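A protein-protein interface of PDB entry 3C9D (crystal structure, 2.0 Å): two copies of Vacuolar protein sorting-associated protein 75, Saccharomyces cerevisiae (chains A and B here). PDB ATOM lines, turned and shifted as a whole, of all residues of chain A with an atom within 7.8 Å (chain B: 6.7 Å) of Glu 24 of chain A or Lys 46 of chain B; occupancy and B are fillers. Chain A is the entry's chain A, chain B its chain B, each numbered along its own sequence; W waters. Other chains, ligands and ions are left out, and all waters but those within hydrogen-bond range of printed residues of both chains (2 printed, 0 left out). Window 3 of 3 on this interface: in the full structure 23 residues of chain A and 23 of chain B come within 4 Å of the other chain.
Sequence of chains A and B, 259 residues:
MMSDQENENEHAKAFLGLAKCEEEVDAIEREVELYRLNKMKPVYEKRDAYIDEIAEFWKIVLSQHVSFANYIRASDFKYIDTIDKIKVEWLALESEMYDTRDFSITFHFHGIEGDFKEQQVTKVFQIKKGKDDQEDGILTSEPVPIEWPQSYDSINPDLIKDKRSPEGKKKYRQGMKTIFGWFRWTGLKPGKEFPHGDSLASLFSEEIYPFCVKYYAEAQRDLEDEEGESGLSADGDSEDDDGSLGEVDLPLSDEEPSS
The side-chain sulfur (SG) of Cys 21 of chain A sits close to the backbone NH (N) of Arg 47 of chain B (3.8 Å).
NZ of Lys 46 of chain B lies within salt-bridge range of OE2 of Glu 24 of chain A.
SG of Cys 21 of chain A is in hydrogen-bond range of O of Gly 17 of chain A, 3.4 Å away.
The guanidinium group (NE) of Arg 47 of chain B lies within salt-bridge range of the side-chain carboxylate (OD1) of Asp 48 of chain B, at 3.1 Å.
Ala 14 of chain A touches Tyr 50 of chain B.
Gly 17 of chain A touches Tyr 50 of chain B (CA to CZ, 3.6 Å).
CD2 of Leu 18 of chain A touches O of Arg 47 of chain B, 3.6 Å away.
CD2 of Leu 18 of chain A touches CB of Tyr 50 of chain B, 3.8 Å away.
CG2 of Val 43 of chain B touches OE1 of Glu 24 of chain A, 3.6 Å away.
Val 25 of chain A touches Met 40 of chain B.
Met 40 of chain B touches Ile 28 of chain A.
Ile 28 of chain A touches Val 43 of chain B.
Of the printed residues of chain B, Gly 17 of chain A touches Tyr 50 (3.6 Å).
Of the printed residues of chain B, Leu 18 of chain A touches Arg 47 and Tyr 50.
Glu 24 of chain A touches just these residues of chain B: Val 43 and Lys 46.
Printed residues of chain B within 4 Å of Val 25 of chain A: Met 40 (3.7 Å).
Asp 26 of chain A touches none of the printed residues of chain B.
Printed residues of chain A within 4 Å of Met 40 of chain B: Val 25 (3.7 Å) and Ile 28 (3.7 Å).
Of the printed residues of chain A, Val 43 of chain B touches Glu 24 and Ile 28.
Glu 45 of chain B touches none of the printed residues of chain A.
Of the printed residues of chain A, Lys 46 of chain B touches Glu 24.
The nearest residue of chain A that does not touch Lys 46 of chain B is Cys 21 of chain A (4.1 Å).
The nearest printed residue of chain A that does not touch Met 40 of chain B is Glu 24 of chain A (5.8 Å).
Printed residues of chain B that touch a printed residue of chain A: Met 40, Val 43, Lys 46, Arg 47 and Tyr 50.
No position is printed for both chains.
Of the 10 pairs that touch across the chains among the printed residues, none has its exchanged pair printed and touching as well.
Water W1 lies within hydrogen-bond range of OE2 of Glu 29 of chain A (2.8 Å) and SD of Met 40 of chain B (3.7 Å).
Water W2 bridges OE1 of Glu 24 of chain A (3.4 Å) and NZ of Lys 46 of chain B (3.4 Å).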
ATOM      1  N   ALA A  14      26.130 -28.217  28.376  1.00  0.00           N
ATOM      2  CA  ALA A  14      25.093 -27.669  27.512  1.00  0.00           C
ATOM      3  C   ALA A  14      23.723 -27.699  28.193  1.00  0.00           C
ATOM      4  O   ALA A  14      22.965 -26.728  28.110  1.00  0.00           O
ATOM      5  CB  ALA A  14      25.056 -28.424  26.184  1.00  0.00           C
ATOM      6  N   GLY A  17      23.539 -25.004  30.868  1.00  0.00           N
ATOM      7  CA  GLY A  17      23.346 -23.754  30.140  1.00  0.00           C
ATOM      8  C   GLY A  17      21.914 -23.585  29.662  1.00  0.00           C
ATOM      9  O   GLY A  17      21.337 -22.495  29.780  1.00  0.00           O
ATOM     10  N   LEU A  18      21.326 -24.668  29.144  1.00  0.00           N
ATOM     11  CA  LEU A  18      19.932 -24.633  28.671  1.00  0.00           C
ATOM     12  C   LEU A  18      18.904 -24.472  29.793  1.00  0.00           C
ATOM     13  O   LEU A  18      17.881 -23.796  29.616  1.00  0.00           O
ATOM     14  CB  LEU A  18      19.605 -25.863  27.821  1.00  0.00           C
ATOM     15  CG  LEU A  18      20.314 -25.984  26.463  1.00  0.00           C
ATOM     16  CD1 LEU A  18      19.924 -27.289  25.789  1.00  0.00           C
ATOM     17  CD2 LEU A  18      20.017 -24.782  25.558  1.00  0.00           C
ATOM     18  N   ALA A  19      19.171 -25.096  30.942  1.00  0.00           N
ATOM     19  CA  ALA A  19      18.300 -24.955  32.107  1.00  0.00           C
ATOM     20  C   ALA A  19      18.211 -23.493  32.540  1.00  0.00           C
ATOM     21  O   ALA A  19      17.122 -22.992  32.853  1.00  0.00           O
ATOM     22  CB  ALA A  19      18.797 -25.842  33.273  1.00  0.00           C
ATOM     23  N   LYS A  20      19.354 -22.807  32.539  1.00  0.00           N
ATOM     24  CA  LYS A  20      19.416 -21.397  32.922  1.00  0.00           C
ATOM     25  C   LYS A  20      18.741 -20.500  31.889  1.00  0.00           C
ATOM     26  O   LYS A  20      18.047 -19.546  32.245  1.00  0.00           O
ATOM     27  CB  LYS A  20      20.865 -20.959  33.131  1.00  0.00           C
ATOM     28  CG  LYS A  20      21.528 -21.571  34.348  1.00  0.00           C
ATOM     29  CD  LYS A  20      23.005 -21.193  34.406  1.00  0.00           C
ATOM     30  CE  LYS A  20      23.644 -21.687  35.692  1.00  0.00           C
ATOM     31  NZ  LYS A  20      25.100 -21.403  35.722  1.00  0.00           N
ATOM     32  N   CYS A  21      18.934 -20.809  30.609  1.00  0.00           N
ATOM     33  CA  CYS A  21      18.245 -20.072  29.549  1.00  0.00           C
ATOM     34  C   CYS A  21      16.733 -20.158  29.708  1.00  0.00           C
ATOM     35  O   CYS A  21      16.033 -19.177  29.488  1.00  0.00           O
ATOM     36  CB  CYS A  21      18.652 -20.574  28.172  1.00  0.00           C
ATOM     37  SG  CYS A  21      20.304 -20.085  27.680  1.00  0.00           S
ATOM     38  N   GLU A  22      16.240 -21.335  30.110  1.00  0.00           N
ATOM     39  CA  GLU A  22      14.799 -21.557  30.274  1.00  0.00           C
ATOM     40  C   GLU A  22      14.219 -20.741  31.435  1.00  0.00           C
ATOM     41  O   GLU A  22      13.089 -20.257  31.359  1.00  0.00           O
ATOM     42  CB  GLU A  22      14.488 -23.043  30.475  1.00  0.00           C
ATOM     43  CG  GLU A  22      14.807 -23.933  29.273  1.00  0.00           C
ATOM     44  CD  GLU A  22      14.148 -23.468  27.978  1.00  0.00           C
ATOM     45  OE1 GLU A  22      13.146 -22.715  28.028  1.00  0.00           O
ATOM     46  OE2 GLU A  22      14.641 -23.857  26.901  1.00  0.00           O
ATOM     47  N   GLU A  23      14.997 -20.596  32.500  1.00  0.00           N
ATOM     48  CA  GLU A  23      14.607 -19.734  33.617  1.00  0.00           C
ATOM     49  C   GLU A  23      14.533 -18.269  33.164  1.00  0.00           C
ATOM     50  O   GLU A  23      13.604 -17.562  33.525  1.00  0.00           O
ATOM     51  CB  GLU A  23      15.567 -19.889  34.809  1.00  0.00           C
ATOM     52  CG  GLU A  23      15.671 -21.329  35.377  1.00  0.00           C
ATOM     53  CD  GLU A  23      14.352 -21.874  35.975  1.00  0.00           C
ATOM     54  OE1 GLU A  23      13.325 -21.158  35.982  1.00  0.00           O
ATOM     55  OE2 GLU A  23      14.353 -23.037  36.446  1.00  0.00           O
ATOM     56  N   GLU A  24      15.501 -17.837  32.351  1.00  0.00           N
ATOM     57  CA  GLU A  24      15.487 -16.471  31.794  1.00  0.00           C
ATOM     58  C   GLU A  24      14.263 -16.205  30.922  1.00  0.00           C
ATOM     59  O   GLU A  24      13.696 -15.114  30.960  1.00  0.00           O
ATOM     60  CB  GLU A  24      16.769 -16.172  31.005  1.00  0.00           C
ATOM     61  CG  GLU A  24      18.042 -16.269  31.834  1.00  0.00           C
ATOM     62  CD  GLU A  24      19.152 -15.377  31.315  1.00  0.00           C
ATOM     63  OE1 GLU A  24      18.998 -14.780  30.220  1.00  0.00           O
ATOM     64  OE2 GLU A  24      20.186 -15.263  32.010  1.00  0.00           O
ATOM     65  N   VAL A  25      13.868 -17.202  30.134  1.00  0.00           N
ATOM     66  CA  VAL A  25      12.654 -17.123  29.311  1.00  0.00           C
ATOM     67  C   VAL A  25      11.392 -16.922  30.180  1.00  0.00           C
ATOM     68  O   VAL A  25      10.546 -16.060  29.884  1.00  0.00           O
ATOM     69  CB  VAL A  25      12.504 -18.394  28.428  1.00  0.00           C
ATOM     70  CG1 VAL A  25      11.122 -18.467  27.810  1.00  0.00           C
ATOM     71  CG2 VAL A  25      13.593 -18.433  27.353  1.00  0.00           C
ATOM     72  N   ASP A  26      11.288 -17.708  31.256  1.00  0.00           N
ATOM     73  CA  ASP A  26      10.189 -17.581  32.222  1.00  0.00           C
ATOM     74  C   ASP A  26      10.142 -16.195  32.837  1.00  0.00           C
ATOM     75  O   ASP A  26       9.080 -15.591  32.926  1.00  0.00           O
ATOM     76  CB  ASP A  26      10.317 -18.628  33.329  1.00  0.00           C
ATOM     77  CG  ASP A  26      10.026 -20.035  32.840  1.00  0.00           C
ATOM     78  OD1 ASP A  26       9.564 -20.189  31.686  1.00  0.00           O
ATOM     79  OD2 ASP A  26      10.259 -20.990  33.612  1.00  0.00           O
ATOM     80  N   ALA A  27      11.302 -15.702  33.273  1.00  0.00           N
ATOM     81  CA  ALA A  27      11.417 -14.350  33.803  1.00  0.00           C
ATOM     82  C   ALA A  27      10.927 -13.318  32.782  1.00  0.00           C
ATOM     83  O   ALA A  27      10.175 -12.419  33.124  1.00  0.00           O
ATOM     84  CB  ALA A  27      12.864 -14.059  34.228  1.00  0.00           C
ATOM     85  N   ILE A  28      11.348 -13.471  31.524  1.00  0.00           N
ATOM     86  CA  ILE A  28      10.897 -12.590  30.446  1.00  0.00           C
ATOM     87  C   ILE A  28       9.379 -12.646  30.222  1.00  0.00           C
ATOM     88  O   ILE A  28       8.734 -11.603  30.092  1.00  0.00           O
ATOM     89  CB  ILE A  28      11.648 -12.861  29.114  1.00  0.00           C
ATOM     90  CG1 ILE A  28      13.119 -12.452  29.239  1.00  0.00           C
ATOM     91  CG2 ILE A  28      10.981 -12.114  27.950  1.00  0.00           C
ATOM     92  CD1 ILE A  28      14.032 -13.072  28.169  1.00  0.00           C
ATOM     93  N   GLU A  29       8.816 -13.855  30.181  1.00  0.00           N
ATOM     94  CA  GLU A  29       7.381 -14.018  29.920  1.00  0.00           C
ATOM     95  C   GLU A  29       6.546 -13.305  30.986  1.00  0.00           C
ATOM     96  O   GLU A  29       5.533 -12.694  30.676  1.00  0.00           O
ATOM     97  CB  GLU A  29       6.986 -15.501  29.846  1.00  0.00           C
ATOM     98  CG  GLU A  29       7.499 -16.252  28.616  1.00  0.00           C
ATOM     99  CD  GLU A  29       6.733 -15.940  27.327  1.00  0.00           C
ATOM    100  OE1 GLU A  29       5.952 -14.962  27.289  1.00  0.00           O
ATOM    101  OE2 GLU A  29       6.926 -16.682  26.332  1.00  0.00           O
ATOM    102  N   ARG A  30       6.986 -13.386  32.237  1.00  0.00           N
ATOM    103  CA  ARG A  30       6.312 -12.682  33.327  1.00  0.00           C
ATOM    104  C   ARG A  30       6.361 -11.157  33.139  1.00  0.00           C
ATOM    105  O   ARG A  30       5.328 -10.480  33.217  1.00  0.00           O
ATOM    106  CB  ARG A  30       6.901 -13.071  34.688  1.00  0.00           C
ATOM    107  CG  ARG A  30       6.091 -12.507  35.841  1.00  0.00           C
ATOM    108  CD  ARG A  30       6.795 -12.596  37.174  1.00  0.00           C
ATOM    109  NE  ARG A  30       6.265 -11.576  38.085  1.00  0.00           N
ATOM    110  CZ  ARG A  30       5.107 -11.668  38.743  1.00  0.00           C
ATOM    111  NH1 ARG A  30       4.340 -12.747  38.625  1.00  0.00           N
ATOM    112  NH2 ARG A  30       4.715 -10.673  39.524  1.00  0.00           N
ATOM    113  N   MET B  40      14.145 -11.343  24.034  1.00  0.00           N
ATOM    114  CA  MET B  40      14.490 -12.738  23.718  1.00  0.00           C
ATOM    115  C   MET B  40      15.747 -12.891  22.870  1.00  0.00           C
ATOM    116  O   MET B  40      16.382 -13.941  22.894  1.00  0.00           O
ATOM    117  CB  MET B  40      13.318 -13.451  23.022  1.00  0.00           C
ATOM    118  CG  MET B  40      12.216 -13.896  23.955  1.00  0.00           C
ATOM    119  SD  MET B  40      12.774 -15.012  25.256  1.00  0.00           S
ATOM    120  CE  MET B  40      13.656 -16.253  24.304  1.00  0.00           C
ATOM    121  N   LYS B  41      16.095 -11.854  22.112  1.00  0.00           N
ATOM    122  CA  LYS B  41      17.165 -11.958  21.123  1.00  0.00           C
ATOM    123  C   LYS B  41      18.486 -12.432  21.726  1.00  0.00           C
ATOM    124  O   LYS B  41      19.046 -13.412  21.254  1.00  0.00           O
ATOM    125  CB  LYS B  41      17.375 -10.630  20.367  1.00  0.00           C
ATOM    126  CG  LYS B  41      18.313 -10.755  19.168  1.00  0.00           C
ATOM    127  CD  LYS B  41      18.523  -9.420  18.482  1.00  0.00           C
ATOM    128  CE  LYS B  41      19.513  -9.545  17.333  1.00  0.00           C
ATOM    129  NZ  LYS B  41      19.813  -8.204  16.737  1.00  0.00           N
ATOM    130  N   PRO B  42      18.987 -11.736  22.772  1.00  0.00           N
ATOM    131  CA  PRO B  42      20.227 -12.195  23.405  1.00  0.00           C
ATOM    132  C   PRO B  42      20.095 -13.570  24.072  1.00  0.00           C
ATOM    133  O   PRO B  42      21.067 -14.329  24.120  1.00  0.00           O
ATOM    134  CB  PRO B  42      20.515 -11.113  24.459  1.00  0.00           C
ATOM    135  CG  PRO B  42      19.228 -10.414  24.682  1.00  0.00           C
ATOM    136  CD  PRO B  42      18.477 -10.492  23.394  1.00  0.00           C
ATOM    137  N   VAL B  43      18.903 -13.888  24.573  1.00  0.00           N
ATOM    138  CA  VAL B  43      18.674 -15.182  25.207  1.00  0.00           C
ATOM    139  C   VAL B  43      18.733 -16.300  24.175  1.00  0.00           C
ATOM    140  O   VAL B  43      19.368 -17.334  24.403  1.00  0.00           O
ATOM    141  CB  VAL B  43      17.324 -15.229  25.947  1.00  0.00           C
ATOM    142  CG1 VAL B  43      17.071 -16.621  26.506  1.00  0.00           C
ATOM    143  CG2 VAL B  43      17.293 -14.169  27.064  1.00  0.00           C
ATOM    144  N   TYR B  44      18.061 -16.089  23.045  1.00  0.00           N
ATOM    145  CA  TYR B  44      18.104 -17.038  21.943  1.00  0.00           C
ATOM    146  C   TYR B  44      19.539 -17.288  21.485  1.00  0.00           C
ATOM    147  O   TYR B  44      19.922 -18.428  21.251  1.00  0.00           O
ATOM    148  CB  TYR B  44      17.241 -16.553  20.771  1.00  0.00           C
ATOM    149  CG  TYR B  44      15.771 -16.903  20.875  1.00  0.00           C
ATOM    150  CD1 TYR B  44      14.792 -15.990  20.486  1.00  0.00           C
ATOM    151  CD2 TYR B  44      15.356 -18.157  21.335  1.00  0.00           C
ATOM    152  CE1 TYR B  44      13.440 -16.305  20.566  1.00  0.00           C
ATOM    153  CE2 TYR B  44      14.005 -18.481  21.420  1.00  0.00           C
ATOM    154  CZ  TYR B  44      13.056 -17.551  21.032  1.00  0.00           C
ATOM    155  OH  TYR B  44      11.727 -17.862  21.111  1.00  0.00           O
ATOM    156  N   GLU B  45      20.335 -16.218  21.390  1.00  0.00           N
ATOM    157  CA  GLU B  45      21.750 -16.311  20.986  1.00  0.00           C
ATOM    158  C   GLU B  45      22.581 -17.203  21.913  1.00  0.00           C
ATOM    159  O   GLU B  45      23.304 -18.076  21.451  1.00  0.00           O
ATOM    160  CB  GLU B  45      22.383 -14.915  20.889  1.00  0.00           C
ATOM    161  CG  GLU B  45      21.873 -14.084  19.713  1.00  0.00           C
ATOM    162  CD  GLU B  45      22.545 -12.717  19.609  1.00  0.00           C
ATOM    163  OE1 GLU B  45      23.351 -12.370  20.504  1.00  0.00           O
ATOM    164  OE2 GLU B  45      22.267 -11.990  18.629  1.00  0.00           O
ATOM    165  N   LYS B  46      22.464 -16.989  23.219  1.00  0.00           N
ATOM    166  CA  LYS B  46      23.151 -17.848  24.189  1.00  0.00           C
ATOM    167  C   LYS B  46      22.610 -19.284  24.142  1.00  0.00           C
ATOM    168  O   LYS B  46      23.383 -20.245  24.158  1.00  0.00           O
ATOM    169  CB  LYS B  46      23.018 -17.284  25.600  1.00  0.00           C
ATOM    170  CG  LYS B  46      23.852 -18.021  26.630  1.00  0.00           C
ATOM    171  CD  LYS B  46      23.484 -17.601  28.050  1.00  0.00           C
ATOM    172  CE  LYS B  46      23.005 -16.161  28.083  1.00  0.00           C
ATOM    173  NZ  LYS B  46      23.169 -15.555  29.439  1.00  0.00           N
ATOM    174  N   ARG B  47      21.285 -19.416  24.076  1.00  0.00           N
ATOM    175  CA  ARG B  47      20.616 -20.729  23.987  1.00  0.00           C
ATOM    176  C   ARG B  47      21.113 -21.553  22.797  1.00  0.00           C
ATOM    177  O   ARG B  47      21.462 -22.732  22.950  1.00  0.00           O
ATOM    178  CB  ARG B  47      19.097 -20.559  23.889  1.00  0.00           C
ATOM    179  CG  ARG B  47      18.317 -21.876  23.953  1.00  0.00           C
ATOM    180  CD  ARG B  47      16.898 -21.715  23.458  1.00  0.00           C
ATOM    181  NE  ARG B  47      16.825 -21.597  21.999  1.00  0.00           N
ATOM    182  CZ  ARG B  47      15.702 -21.708  21.287  1.00  0.00           C
ATOM    183  NH1 ARG B  47      14.546 -21.951  21.886  1.00  0.00           N
ATOM    184  NH2 ARG B  47      15.739 -21.588  19.963  1.00  0.00           N
ATOM    185  N   ASP B  48      21.143 -20.919  21.622  1.00  0.00           N
ATOM    186  CA  ASP B  48      21.535 -21.589  20.382  1.00  0.00           C
ATOM    187  C   ASP B  48      23.010 -22.006  20.391  1.00  0.00           C
ATOM    188  O   ASP B  48      23.375 -23.020  19.793  1.00  0.00           O
ATOM    189  CB  ASP B  48      21.216 -20.711  19.157  1.00  0.00           C
ATOM    190  CG  ASP B  48      19.697 -20.493  18.956  1.00  0.00           C
ATOM    191  OD1 ASP B  48      18.885 -21.092  19.700  1.00  0.00           O
ATOM    192  OD2 ASP B  48      19.320 -19.720  18.046  1.00  0.00           O
ATOM    193  N   ALA B  49      23.839 -21.225  21.084  1.00  0.00           N
ATOM    194  CA  ALA B  49      25.240 -21.579  21.334  1.00  0.00           C
ATOM    195  C   ALA B  49      25.399 -22.917  22.091  1.00  0.00           C
ATOM    196  O   ALA B  49      26.231 -23.740  21.725  1.00  0.00           O
ATOM    197  CB  ALA B  49      25.960 -20.441  22.076  1.00  0.00           C
ATOM    198  N   TYR B  50      24.598 -23.122  23.137  1.00  0.00           N
ATOM    199  CA  TYR B  50      24.557 -24.410  23.850  1.00  0.00           C
ATOM    200  C   TYR B  50      23.995 -25.540  22.973  1.00  0.00           C
ATOM    201  O   TYR B  50      24.541 -26.654  22.951  1.00  0.00           O
ATOM    202  CB  TYR B  50      23.738 -24.302  25.142  1.00  0.00           C
ATOM    203  CG  TYR B  50      24.352 -23.400  26.197  1.00  0.00           C
ATOM    204  CD1 TYR B  50      23.685 -22.261  26.628  1.00  0.00           C
ATOM    205  CD2 TYR B  50      25.596 -23.692  26.765  1.00  0.00           C
ATOM    206  CE1 TYR B  50      24.233 -21.423  27.595  1.00  0.00           C
ATOM    207  CE2 TYR B  50      26.160 -22.860  27.738  1.00  0.00           C
ATOM    208  CZ  TYR B  50      25.466 -21.724  28.143  1.00  0.00           C
ATOM    209  OH  TYR B  50      25.988 -20.896  29.102  1.00  0.00           O
ATOM    210  N   ILE B  51      22.914 -25.247  22.255  1.00  0.00           N
ATOM    211  CA  ILE B  51      22.309 -26.203  21.323  1.00  0.00           C
ATOM    212  C   ILE B  51      23.330 -26.730  20.311  1.00  0.00           C
ATOM    213  O   ILE B  51      23.329 -27.923  19.973  1.00  0.00           O
ATOM    214  CB  ILE B  51      21.098 -25.583  20.575  1.00  0.00           C
ATOM    215  CG1 ILE B  51      19.901 -25.436  21.523  1.00  0.00           C
ATOM    216  CG2 ILE B  51      20.735 -26.422  19.349  1.00  0.00           C
ATOM    217  CD1 ILE B  51      18.753 -24.619  20.948  1.00  0.00           C
HETATM  218  O   HOH W   1       9.352 -16.320  24.901  1.00  0.00           O
HETATM  219  O   HOH W   2      21.074 -13.268  27.941  1.00  0.00           O
